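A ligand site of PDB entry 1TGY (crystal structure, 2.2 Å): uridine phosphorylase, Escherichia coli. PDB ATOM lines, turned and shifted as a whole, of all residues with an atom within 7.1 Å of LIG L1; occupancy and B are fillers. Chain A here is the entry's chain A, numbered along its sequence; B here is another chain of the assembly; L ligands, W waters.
An oxygen (O6) of LG2 L2 is in salt-bridge range of the guanidinium group of Arg 94.
OE1 of Glu 199 lies within hydrogen-bond range of O3 of LG2 L2 (3.3 Å).
A nitrogen (N2) of LIG L1 sits at hydrogen-bond distance from the side-chain amide oxygen (OE1) of Gln 169, at 2.9 Å.
The guanidinium group (NH1) of Arg 51 of chain B is in salt-bridge range of an oxygen (O7) of LG2 L2 (2.7 Å).
An oxygen (O3) of LG2 L2 is in hydrogen-bond range of the side-chain carboxylate (OE1) of Glu 201 (2.5 Å).
NH2 of Arg 171 lies within hydrogen-bond range of O2 of LIG L1 (2.7 Å).
An oxygen (O3) of LG2 L2 lies within hydrogen-bond range of the backbone NH (N) of Met 200, 2.8 Å away.
The side-chain hydroxyl (OG1) of Thr 97 lies within hydrogen-bond range of an oxygen (O8) of LG2 L2 (2.5 Å).
N of Thr 97 lies within hydrogen-bond range of O8 of LG2 L2 (3.5 Å).
An oxygen (O1) of LG2 L2 sits at hydrogen-bond distance from a ring nitrogen (NE2) of His 11 of chain B, at 2.8 Å.
O of Gly 99 lies within hydrogen-bond range of N of Tyr 198.
The backbone carbonyl oxygen (O) of Glu 199 lies within hydrogen-bond range of the backbone NH (N) of Ser 162, 2.8 Å away.
N of Glu 199 lies within hydrogen-bond range of O of Ala 160 (3.0 Å).
The guanidinium group of Arg 171 sits at hydrogen-bond distance from the side-chain amide oxygen of Gln 169, at 3.0 Å.
NH1 of Arg 226 lies within hydrogen-bond range of O of Gln 169, at 2.8 Å.
The backbone carbonyl oxygen of Thr 164 is in hydrogen-bond range of the side-chain amide nitrogen of Gln 169, at 3.2 Å.
The backbone carbonyl oxygen (O) of Val 224 lies within hydrogen-bond range of the backbone NH (N) of Ala 100 (2.9 Å).
N of Ile 223 sits at hydrogen-bond distance from O of Thr 98, at 3.1 Å.
Merely in contact with LIG L1: Glu 199, Met 200, Phe 165, Val 224, Gly 99, Tyr 198, Thr 97 and Thr 98.
Hydrophobic or aromatic side chains that line LIG L1: Phe 165, Met 200 and Val 224.
The nearest printed residue that does not touch LIG L1 is Ile 223 (4.05 Å).
Water W2 lies within hydrogen-bond range of the guanidinium group of Arg 226 (2.7 Å), the side-chain amide oxygen of Gln 169 (2.7 Å), an oxygen (O2) of LIG L1 (2.9 Å) and the guanidinium group of Arg 171 (3.5 Å).
Water W1 bridges an oxygen (O1) of LG2 L2 and the side-chain hydroxyl (OG1) of Thr 97.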
ATOM      1  N   ARG A  94     -27.191 -15.905  10.018  1.00  0.00           N
ATOM      2  CA  ARG A  94     -26.182 -16.478  10.906  1.00  0.00           C
ATOM      3  C   ARG A  94     -25.772 -15.488  11.970  1.00  0.00           C
ATOM      4  O   ARG A  94     -25.563 -14.298  11.686  1.00  0.00           O
ATOM      5  CB  ARG A  94     -24.931 -16.910  10.123  1.00  0.00           C
ATOM      6  CG  ARG A  94     -23.764 -17.294  11.036  1.00  0.00           C
ATOM      7  CD  ARG A  94     -22.567 -17.858  10.266  1.00  0.00           C
ATOM      8  NE  ARG A  94     -21.293 -17.486  10.887  1.00  0.00           N
ATOM      9  CZ  ARG A  94     -20.887 -17.864  12.093  1.00  0.00           C
ATOM     10  NH1 ARG A  94     -21.650 -18.662  12.833  1.00  0.00           N
ATOM     11  NH2 ARG A  94     -19.735 -17.426  12.581  1.00  0.00           N
ATOM     12  N   THR A  97     -19.649 -15.745  16.577  1.00  0.00           N
ATOM     13  CA  THR A  97     -18.599 -15.054  17.308  1.00  0.00           C
ATOM     14  C   THR A  97     -17.485 -14.805  16.290  1.00  0.00           C
ATOM     15  O   THR A  97     -17.405 -15.489  15.267  1.00  0.00           O
ATOM     16  CB  THR A  97     -18.062 -15.903  18.480  1.00  0.00           C
ATOM     17  OG1 THR A  97     -17.695 -17.207  18.007  1.00  0.00           O
ATOM     18  CG2 THR A  97     -19.139 -16.027  19.565  1.00  0.00           C
ATOM     19  N   THR A  98     -16.629 -13.824  16.567  1.00  0.00           N
ATOM     20  CA  THR A  98     -15.572 -13.528  15.617  1.00  0.00           C
ATOM     21  C   THR A  98     -14.377 -12.820  16.228  1.00  0.00           C
ATOM     22  O   THR A  98     -14.465 -12.231  17.319  1.00  0.00           O
ATOM     23  CB  THR A  98     -16.148 -12.656  14.475  1.00  0.00           C
ATOM     24  OG1 THR A  98     -15.138 -12.432  13.481  1.00  0.00           O
ATOM     25  CG2 THR A  98     -16.625 -11.303  15.025  1.00  0.00           C
ATOM     26  N   GLY A  99     -13.244 -12.892  15.532  1.00  0.00           N
ATOM     27  CA  GLY A  99     -12.049 -12.237  15.988  1.00  0.00           C
ATOM     28  C   GLY A  99     -11.776 -11.088  15.037  1.00  0.00           C
ATOM     29  O   GLY A  99     -11.569 -11.312  13.844  1.00  0.00           O
ATOM     30  N   ALA A 100     -11.790  -9.860  15.545  1.00  0.00           N
ATOM     31  CA  ALA A 100     -11.553  -8.693  14.711  1.00  0.00           C
ATOM     32  C   ALA A 100     -10.048  -8.548  14.415  1.00  0.00           C
ATOM     33  O   ALA A 100      -9.216  -8.990  15.200  1.00  0.00           O
ATOM     34  CB  ALA A 100     -12.066  -7.434  15.399  1.00  0.00           C
ATOM     35  N   ALA A 160     -13.206 -12.331   6.539  1.00  0.00           N
ATOM     36  CA  ALA A 160     -12.377 -13.433   6.047  1.00  0.00           C
ATOM     37  C   ALA A 160     -12.916 -14.697   6.709  1.00  0.00           C
ATOM     38  O   ALA A 160     -12.806 -14.858   7.927  1.00  0.00           O
ATOM     39  CB  ALA A 160     -10.919 -13.210   6.438  1.00  0.00           C
ATOM     40  N   SER A 162     -12.564 -18.541   7.167  1.00  0.00           N
ATOM     41  CA  SER A 162     -11.579 -19.615   7.082  1.00  0.00           C
ATOM     42  C   SER A 162     -12.041 -21.032   7.487  1.00  0.00           C
ATOM     43  O   SER A 162     -12.770 -21.196   8.478  1.00  0.00           O
ATOM     44  CB  SER A 162     -10.360 -19.214   7.925  1.00  0.00           C
ATOM     45  OG  SER A 162      -9.384 -20.252   8.018  1.00  0.00           O
ATOM     46  N   THR A 164     -10.293 -22.975   8.737  1.00  0.00           N
ATOM     47  CA  THR A 164      -9.441 -23.275   9.866  1.00  0.00           C
ATOM     48  C   THR A 164      -9.453 -22.177  10.935  1.00  0.00           C
ATOM     49  O   THR A 164      -9.586 -20.996  10.634  1.00  0.00           O
ATOM     50  CB  THR A 164      -8.002 -23.497   9.340  1.00  0.00           C
ATOM     51  OG1 THR A 164      -7.725 -24.903   9.290  1.00  0.00           O
ATOM     52  CG2 THR A 164      -7.000 -22.791  10.170  1.00  0.00           C
ATOM     53  N   PHE A 165      -9.320 -22.584  12.198  1.00  0.00           N
ATOM     54  CA  PHE A 165      -9.293 -21.640  13.308  1.00  0.00           C
ATOM     55  C   PHE A 165      -7.860 -21.165  13.528  1.00  0.00           C
ATOM     56  O   PHE A 165      -7.633 -20.025  13.935  1.00  0.00           O
ATOM     57  CB  PHE A 165      -9.805 -22.295  14.584  1.00  0.00           C
ATOM     58  CG  PHE A 165      -9.873 -21.356  15.762  1.00  0.00           C
ATOM     59  CD1 PHE A 165     -10.985 -20.535  15.939  1.00  0.00           C
ATOM     60  CD2 PHE A 165      -8.828 -21.268  16.662  1.00  0.00           C
ATOM     61  CE1 PHE A 165     -11.055 -19.643  17.016  1.00  0.00           C
ATOM     62  CE2 PHE A 165      -8.871 -20.382  17.745  1.00  0.00           C
ATOM     63  CZ  PHE A 165      -9.993 -19.571  17.924  1.00  0.00           C
ATOM     64  N   GLN A 169      -6.110 -18.513   9.968  1.00  0.00           N
ATOM     65  CA  GLN A 169      -6.280 -17.232  10.644  1.00  0.00           C
ATOM     66  C   GLN A 169      -4.903 -16.795  11.141  1.00  0.00           C
ATOM     67  O   GLN A 169      -4.776 -15.975  12.050  1.00  0.00           O
ATOM     68  CB  GLN A 169      -7.275 -17.378  11.805  1.00  0.00           C
ATOM     69  CG  GLN A 169      -8.704 -17.679  11.353  1.00  0.00           C
ATOM     70  CD  GLN A 169      -9.721 -17.645  12.485  1.00  0.00           C
ATOM     71  OE1 GLN A 169      -9.649 -16.786  13.378  1.00  0.00           O
ATOM     72  NE2 GLN A 169     -10.671 -18.574  12.460  1.00  0.00           N
ATOM     73  N   ARG A 171      -2.480 -18.118  13.036  1.00  0.00           N
ATOM     74  CA  ARG A 171      -2.137 -18.220  14.452  1.00  0.00           C
ATOM     75  C   ARG A 171      -0.863 -19.065  14.504  1.00  0.00           C
ATOM     76  O   ARG A 171      -0.768 -20.075  13.811  1.00  0.00           O
ATOM     77  CB  ARG A 171      -3.258 -18.921  15.236  1.00  0.00           C
ATOM     78  CG  ARG A 171      -4.494 -18.072  15.509  1.00  0.00           C
ATOM     79  CD  ARG A 171      -5.354 -18.694  16.618  1.00  0.00           C
ATOM     80  NE  ARG A 171      -6.187 -17.698  17.288  1.00  0.00           N
ATOM     81  CZ  ARG A 171      -7.339 -17.218  16.812  1.00  0.00           C
ATOM     82  NH1 ARG A 171      -7.815 -17.643  15.643  1.00  0.00           N
ATOM     83  NH2 ARG A 171      -8.004 -16.297  17.495  1.00  0.00           N
ATOM     84  N   TYR A 198     -12.268 -12.405  11.177  1.00  0.00           N
ATOM     85  CA  TYR A 198     -12.114 -13.813  10.801  1.00  0.00           C
ATOM     86  C   TYR A 198     -13.263 -14.586  11.445  1.00  0.00           C
ATOM     87  O   TYR A 198     -13.589 -14.354  12.618  1.00  0.00           O
ATOM     88  CB  TYR A 198     -10.819 -14.414  11.376  1.00  0.00           C
ATOM     89  CG  TYR A 198      -9.539 -14.178  10.609  1.00  0.00           C
ATOM     90  CD1 TYR A 198      -8.432 -13.621  11.234  1.00  0.00           C
ATOM     91  CD2 TYR A 198      -9.404 -14.607   9.278  1.00  0.00           C
ATOM     92  CE1 TYR A 198      -7.213 -13.491  10.574  1.00  0.00           C
ATOM     93  CE2 TYR A 198      -8.184 -14.482   8.602  1.00  0.00           C
ATOM     94  CZ  TYR A 198      -7.090 -13.925   9.262  1.00  0.00           C
ATOM     95  OH  TYR A 198      -5.873 -13.819   8.622  1.00  0.00           O
ATOM     96  N   GLU A 199     -13.875 -15.492  10.686  1.00  0.00           N
ATOM     97  CA  GLU A 199     -14.943 -16.348  11.191  1.00  0.00           C
ATOM     98  C   GLU A 199     -14.820 -17.626  10.360  1.00  0.00           C
ATOM     99  O   GLU A 199     -13.911 -17.715   9.526  1.00  0.00           O
ATOM    100  CB  GLU A 199     -16.311 -15.682  11.027  1.00  0.00           C
ATOM    101  CG  GLU A 199     -16.911 -15.815   9.634  1.00  0.00           C
ATOM    102  CD  GLU A 199     -18.265 -16.453   9.678  1.00  0.00           C
ATOM    103  OE1 GLU A 199     -18.358 -17.615  10.100  1.00  0.00           O
ATOM    104  OE2 GLU A 199     -19.249 -15.794   9.314  1.00  0.00           O
ATOM    105  N   MET A 200     -15.710 -18.597  10.543  1.00  0.00           N
ATOM    106  CA  MET A 200     -15.553 -19.843   9.786  1.00  0.00           C
ATOM    107  C   MET A 200     -16.752 -20.428   9.045  1.00  0.00           C
ATOM    108  O   MET A 200     -16.699 -21.601   8.642  1.00  0.00           O
ATOM    109  CB  MET A 200     -14.968 -20.913  10.719  1.00  0.00           C
ATOM    110  CG  MET A 200     -13.666 -20.513  11.408  1.00  0.00           C
ATOM    111  SD  MET A 200     -13.081 -21.717  12.628  1.00  0.00           S
ATOM    112  CE  MET A 200     -12.585 -23.080  11.548  1.00  0.00           C
ATOM    113  N   GLU A 201     -17.825 -19.662   8.846  1.00  0.00           N
ATOM    114  CA  GLU A 201     -18.990 -20.194   8.130  1.00  0.00           C
ATOM    115  C   GLU A 201     -19.599 -19.274   7.078  1.00  0.00           C
ATOM    116  O   GLU A 201     -20.278 -19.759   6.171  1.00  0.00           O
ATOM    117  CB  GLU A 201     -20.101 -20.600   9.110  1.00  0.00           C
ATOM    118  CG  GLU A 201     -19.791 -21.761  10.065  1.00  0.00           C
ATOM    119  CD  GLU A 201     -18.907 -21.343  11.235  1.00  0.00           C
ATOM    120  OE1 GLU A 201     -19.082 -20.212  11.734  1.00  0.00           O
ATOM    121  OE2 GLU A 201     -18.056 -22.147  11.667  1.00  0.00           O
ATOM    122  N   GLY A 221     -20.565 -11.180  17.034  1.00  0.00           N
ATOM    123  CA  GLY A 221     -20.063 -10.334  18.100  1.00  0.00           C
ATOM    124  C   GLY A 221     -18.577 -10.562  18.267  1.00  0.00           C
ATOM    125  O   GLY A 221     -18.109 -11.706  18.217  1.00  0.00           O
ATOM    126  N   ILE A 223     -15.298 -11.177  20.107  1.00  0.00           N
ATOM    127  CA  ILE A 223     -14.877 -11.697  21.407  1.00  0.00           C
ATOM    128  C   ILE A 223     -13.365 -11.601  21.567  1.00  0.00           C
ATOM    129  O   ILE A 223     -12.804 -12.026  22.584  1.00  0.00           O
ATOM    130  CB  ILE A 223     -15.308 -13.164  21.619  1.00  0.00           C
ATOM    131  CG1 ILE A 223     -14.647 -14.070  20.572  1.00  0.00           C
ATOM    132  CG2 ILE A 223     -16.833 -13.254  21.524  1.00  0.00           C
ATOM    133  CD1 ILE A 223     -14.849 -15.541  20.844  1.00  0.00           C
ATOM    134  N   VAL A 224     -12.699 -11.041  20.567  1.00  0.00           N
ATOM    135  CA  VAL A 224     -11.253 -10.877  20.612  1.00  0.00           C
ATOM    136  C   VAL A 224     -10.815 -10.003  19.447  1.00  0.00           C
ATOM    137  O   VAL A 224     -11.460  -9.974  18.405  1.00  0.00           O
ATOM    138  CB  VAL A 224     -10.511 -12.238  20.505  1.00  0.00           C
ATOM    139  CG1 VAL A 224     -10.710 -12.845  19.124  1.00  0.00           C
ATOM    140  CG2 VAL A 224      -9.033 -12.037  20.782  1.00  0.00           C
ATOM    141  N   ASN A 225      -9.724  -9.274  19.654  1.00  0.00           N
ATOM    142  CA  ASN A 225      -9.190  -8.427  18.604  1.00  0.00           C
ATOM    143  C   ASN A 225      -7.729  -8.807  18.444  1.00  0.00           C
ATOM    144  O   ASN A 225      -6.911  -8.536  19.316  1.00  0.00           O
ATOM    145  CB  ASN A 225      -9.291  -6.945  18.962  1.00  0.00           C
ATOM    146  CG  ASN A 225      -8.824  -6.042  17.828  1.00  0.00           C
ATOM    147  OD1 ASN A 225      -7.785  -6.290  17.228  1.00  0.00           O
ATOM    148  ND2 ASN A 225      -9.591  -4.994  17.541  1.00  0.00           N
ATOM    149  N   ARG A 226      -7.410  -9.450  17.325  1.00  0.00           N
ATOM    150  CA  ARG A 226      -6.062  -9.896  17.054  1.00  0.00           C
ATOM    151  C   ARG A 226      -4.997  -8.787  17.095  1.00  0.00           C
ATOM    152  O   ARG A 226      -3.823  -9.076  17.269  1.00  0.00           O
ATOM    153  CB  ARG A 226      -6.012 -10.602  15.695  1.00  0.00           C
ATOM    154  CG  ARG A 226      -6.932 -11.826  15.603  1.00  0.00           C
ATOM    155  CD  ARG A 226      -6.418 -12.969  16.471  1.00  0.00           C
ATOM    156  NE  ARG A 226      -5.130 -13.471  15.983  1.00  0.00           N
ATOM    157  CZ  ARG A 226      -4.976 -14.175  14.866  1.00  0.00           C
ATOM    158  NH1 ARG A 226      -6.025 -14.491  14.117  1.00  0.00           N
ATOM    159  NH2 ARG A 226      -3.769 -14.553  14.483  1.00  0.00           N
ATOM    160  N   PHE B  10      -8.753 -23.924  23.518  1.00  0.00           N
ATOM    161  CA  PHE B  10      -9.871 -23.048  23.232  1.00  0.00           C
ATOM    162  C   PHE B  10     -11.264 -23.664  23.022  1.00  0.00           C
ATOM    163  O   PHE B  10     -12.257 -23.070  23.430  1.00  0.00           O
ATOM    164  CB  PHE B  10      -9.553 -22.159  22.025  1.00  0.00           C
ATOM    165  CG  PHE B  10     -10.446 -20.957  21.913  1.00  0.00           C
ATOM    166  CD1 PHE B  10     -10.113 -19.755  22.529  1.00  0.00           C
ATOM    167  CD2 PHE B  10     -11.657 -21.044  21.216  1.00  0.00           C
ATOM    168  CE1 PHE B  10     -10.957 -18.650  22.452  1.00  0.00           C
ATOM    169  CE2 PHE B  10     -12.514 -19.937  21.135  1.00  0.00           C
ATOM    170  CZ  PHE B  10     -12.160 -18.744  21.752  1.00  0.00           C
ATOM    171  N   HIS B  11     -11.337 -24.844  22.405  1.00  0.00           N
ATOM    172  CA  HIS B  11     -12.644 -25.442  22.147  1.00  0.00           C
ATOM    173  C   HIS B  11     -13.006 -26.737  22.882  1.00  0.00           C
ATOM    174  O   HIS B  11     -14.147 -26.899  23.312  1.00  0.00           O
ATOM    175  CB  HIS B  11     -12.819 -25.708  20.641  1.00  0.00           C
ATOM    176  CG  HIS B  11     -12.635 -24.508  19.776  1.00  0.00           C
ATOM    177  ND1 HIS B  11     -11.394 -24.053  19.378  1.00  0.00           N
ATOM    178  CD2 HIS B  11     -13.541 -23.672  19.208  1.00  0.00           C
ATOM    179  CE1 HIS B  11     -11.553 -22.995  18.603  1.00  0.00           C
ATOM    180  NE2 HIS B  11     -12.846 -22.741  18.480  1.00  0.00           N
ATOM    181  N   ARG B  51     -19.824 -27.880  22.110  1.00  0.00           N
ATOM    182  CA  ARG B  51     -20.085 -27.779  20.681  1.00  0.00           C
ATOM    183  C   ARG B  51     -20.168 -29.212  20.156  1.00  0.00           C
ATOM    184  O   ARG B  51     -20.786 -30.058  20.792  1.00  0.00           O
ATOM    185  CB  ARG B  51     -18.960 -26.994  19.986  1.00  0.00           C
ATOM    186  CG  ARG B  51     -19.001 -25.477  20.261  1.00  0.00           C
ATOM    187  CD  ARG B  51     -17.767 -24.786  19.701  1.00  0.00           C
ATOM    188  NE  ARG B  51     -17.824 -23.336  19.818  1.00  0.00           N
ATOM    189  CZ  ARG B  51     -18.476 -22.524  18.994  1.00  0.00           C
ATOM    190  NH1 ARG B  51     -19.143 -23.018  17.955  1.00  0.00           N
ATOM    191  NH2 ARG B  51     -18.452 -21.213  19.176  1.00  0.00           N
HETATM  192  N1  LIG L   1     -14.045 -17.343  15.905  1.00  0.00           N
HETATM  193  C1  LIG L   1     -13.093 -17.359  14.855  1.00  0.00           C
HETATM  194  O1  LIG L   1     -13.267 -17.865  13.751  1.00  0.00           O
HETATM  195  N2  LIG L   1     -11.905 -16.720  15.156  1.00  0.00           N
HETATM  196  C2  LIG L   1     -11.539 -16.080  16.358  1.00  0.00           C
HETATM  197  O2  LIG L   1     -10.455 -15.509  16.612  1.00  0.00           O
HETATM  198  C3  LIG L   1     -12.591 -16.123  17.383  1.00  0.00           C
HETATM  199  C4  LIG L   1     -13.776 -16.735  17.128  1.00  0.00           C
HETATM  200  C1  LG2 L   2     -14.662 -20.671  16.129  1.00  0.00           C
HETATM  201  O1  LG2 L   2     -14.446 -20.665  17.545  1.00  0.00           O
HETATM  202  C2  LG2 L   2     -16.162 -20.782  15.859  1.00  0.00           C
HETATM  203  O2  LG2 L   2     -16.907 -19.678  16.407  1.00  0.00           O
HETATM  204  C3  LG2 L   2     -17.282 -18.772  15.345  1.00  0.00           C
HETATM  205  C4  LG2 L   2     -16.545 -19.290  14.108  1.00  0.00           C
HETATM  206  O3  LG2 L   2     -17.210 -18.945  12.894  1.00  0.00           O
HETATM  207  C5  LG2 L   2     -16.509 -20.799  14.366  1.00  0.00           C
HETATM  208  O4  LG2 L   2     -17.809 -21.360  14.176  1.00  0.00           O
HETATM  209  O5  LG2 L   2     -18.694 -18.828  15.119  1.00  0.00           O
HETATM  210  P1  LG2 L   2     -19.701 -19.626  16.088  1.00  0.00           P
HETATM  211  O6  LG2 L   2     -21.097 -19.230  15.765  1.00  0.00           O
HETATM  212  O7  LG2 L   2     -19.349 -21.063  16.078  1.00  0.00           O
HETATM  213  O8  LG2 L   2     -19.347 -19.047  17.550  1.00  0.00           O
HETATM  214  O   HOH W   1     -15.389 -18.746  19.225  1.00  0.00           O
HETATM  215  O   HOH W   2      -8.716 -14.486  14.545  1.00  0.00           O
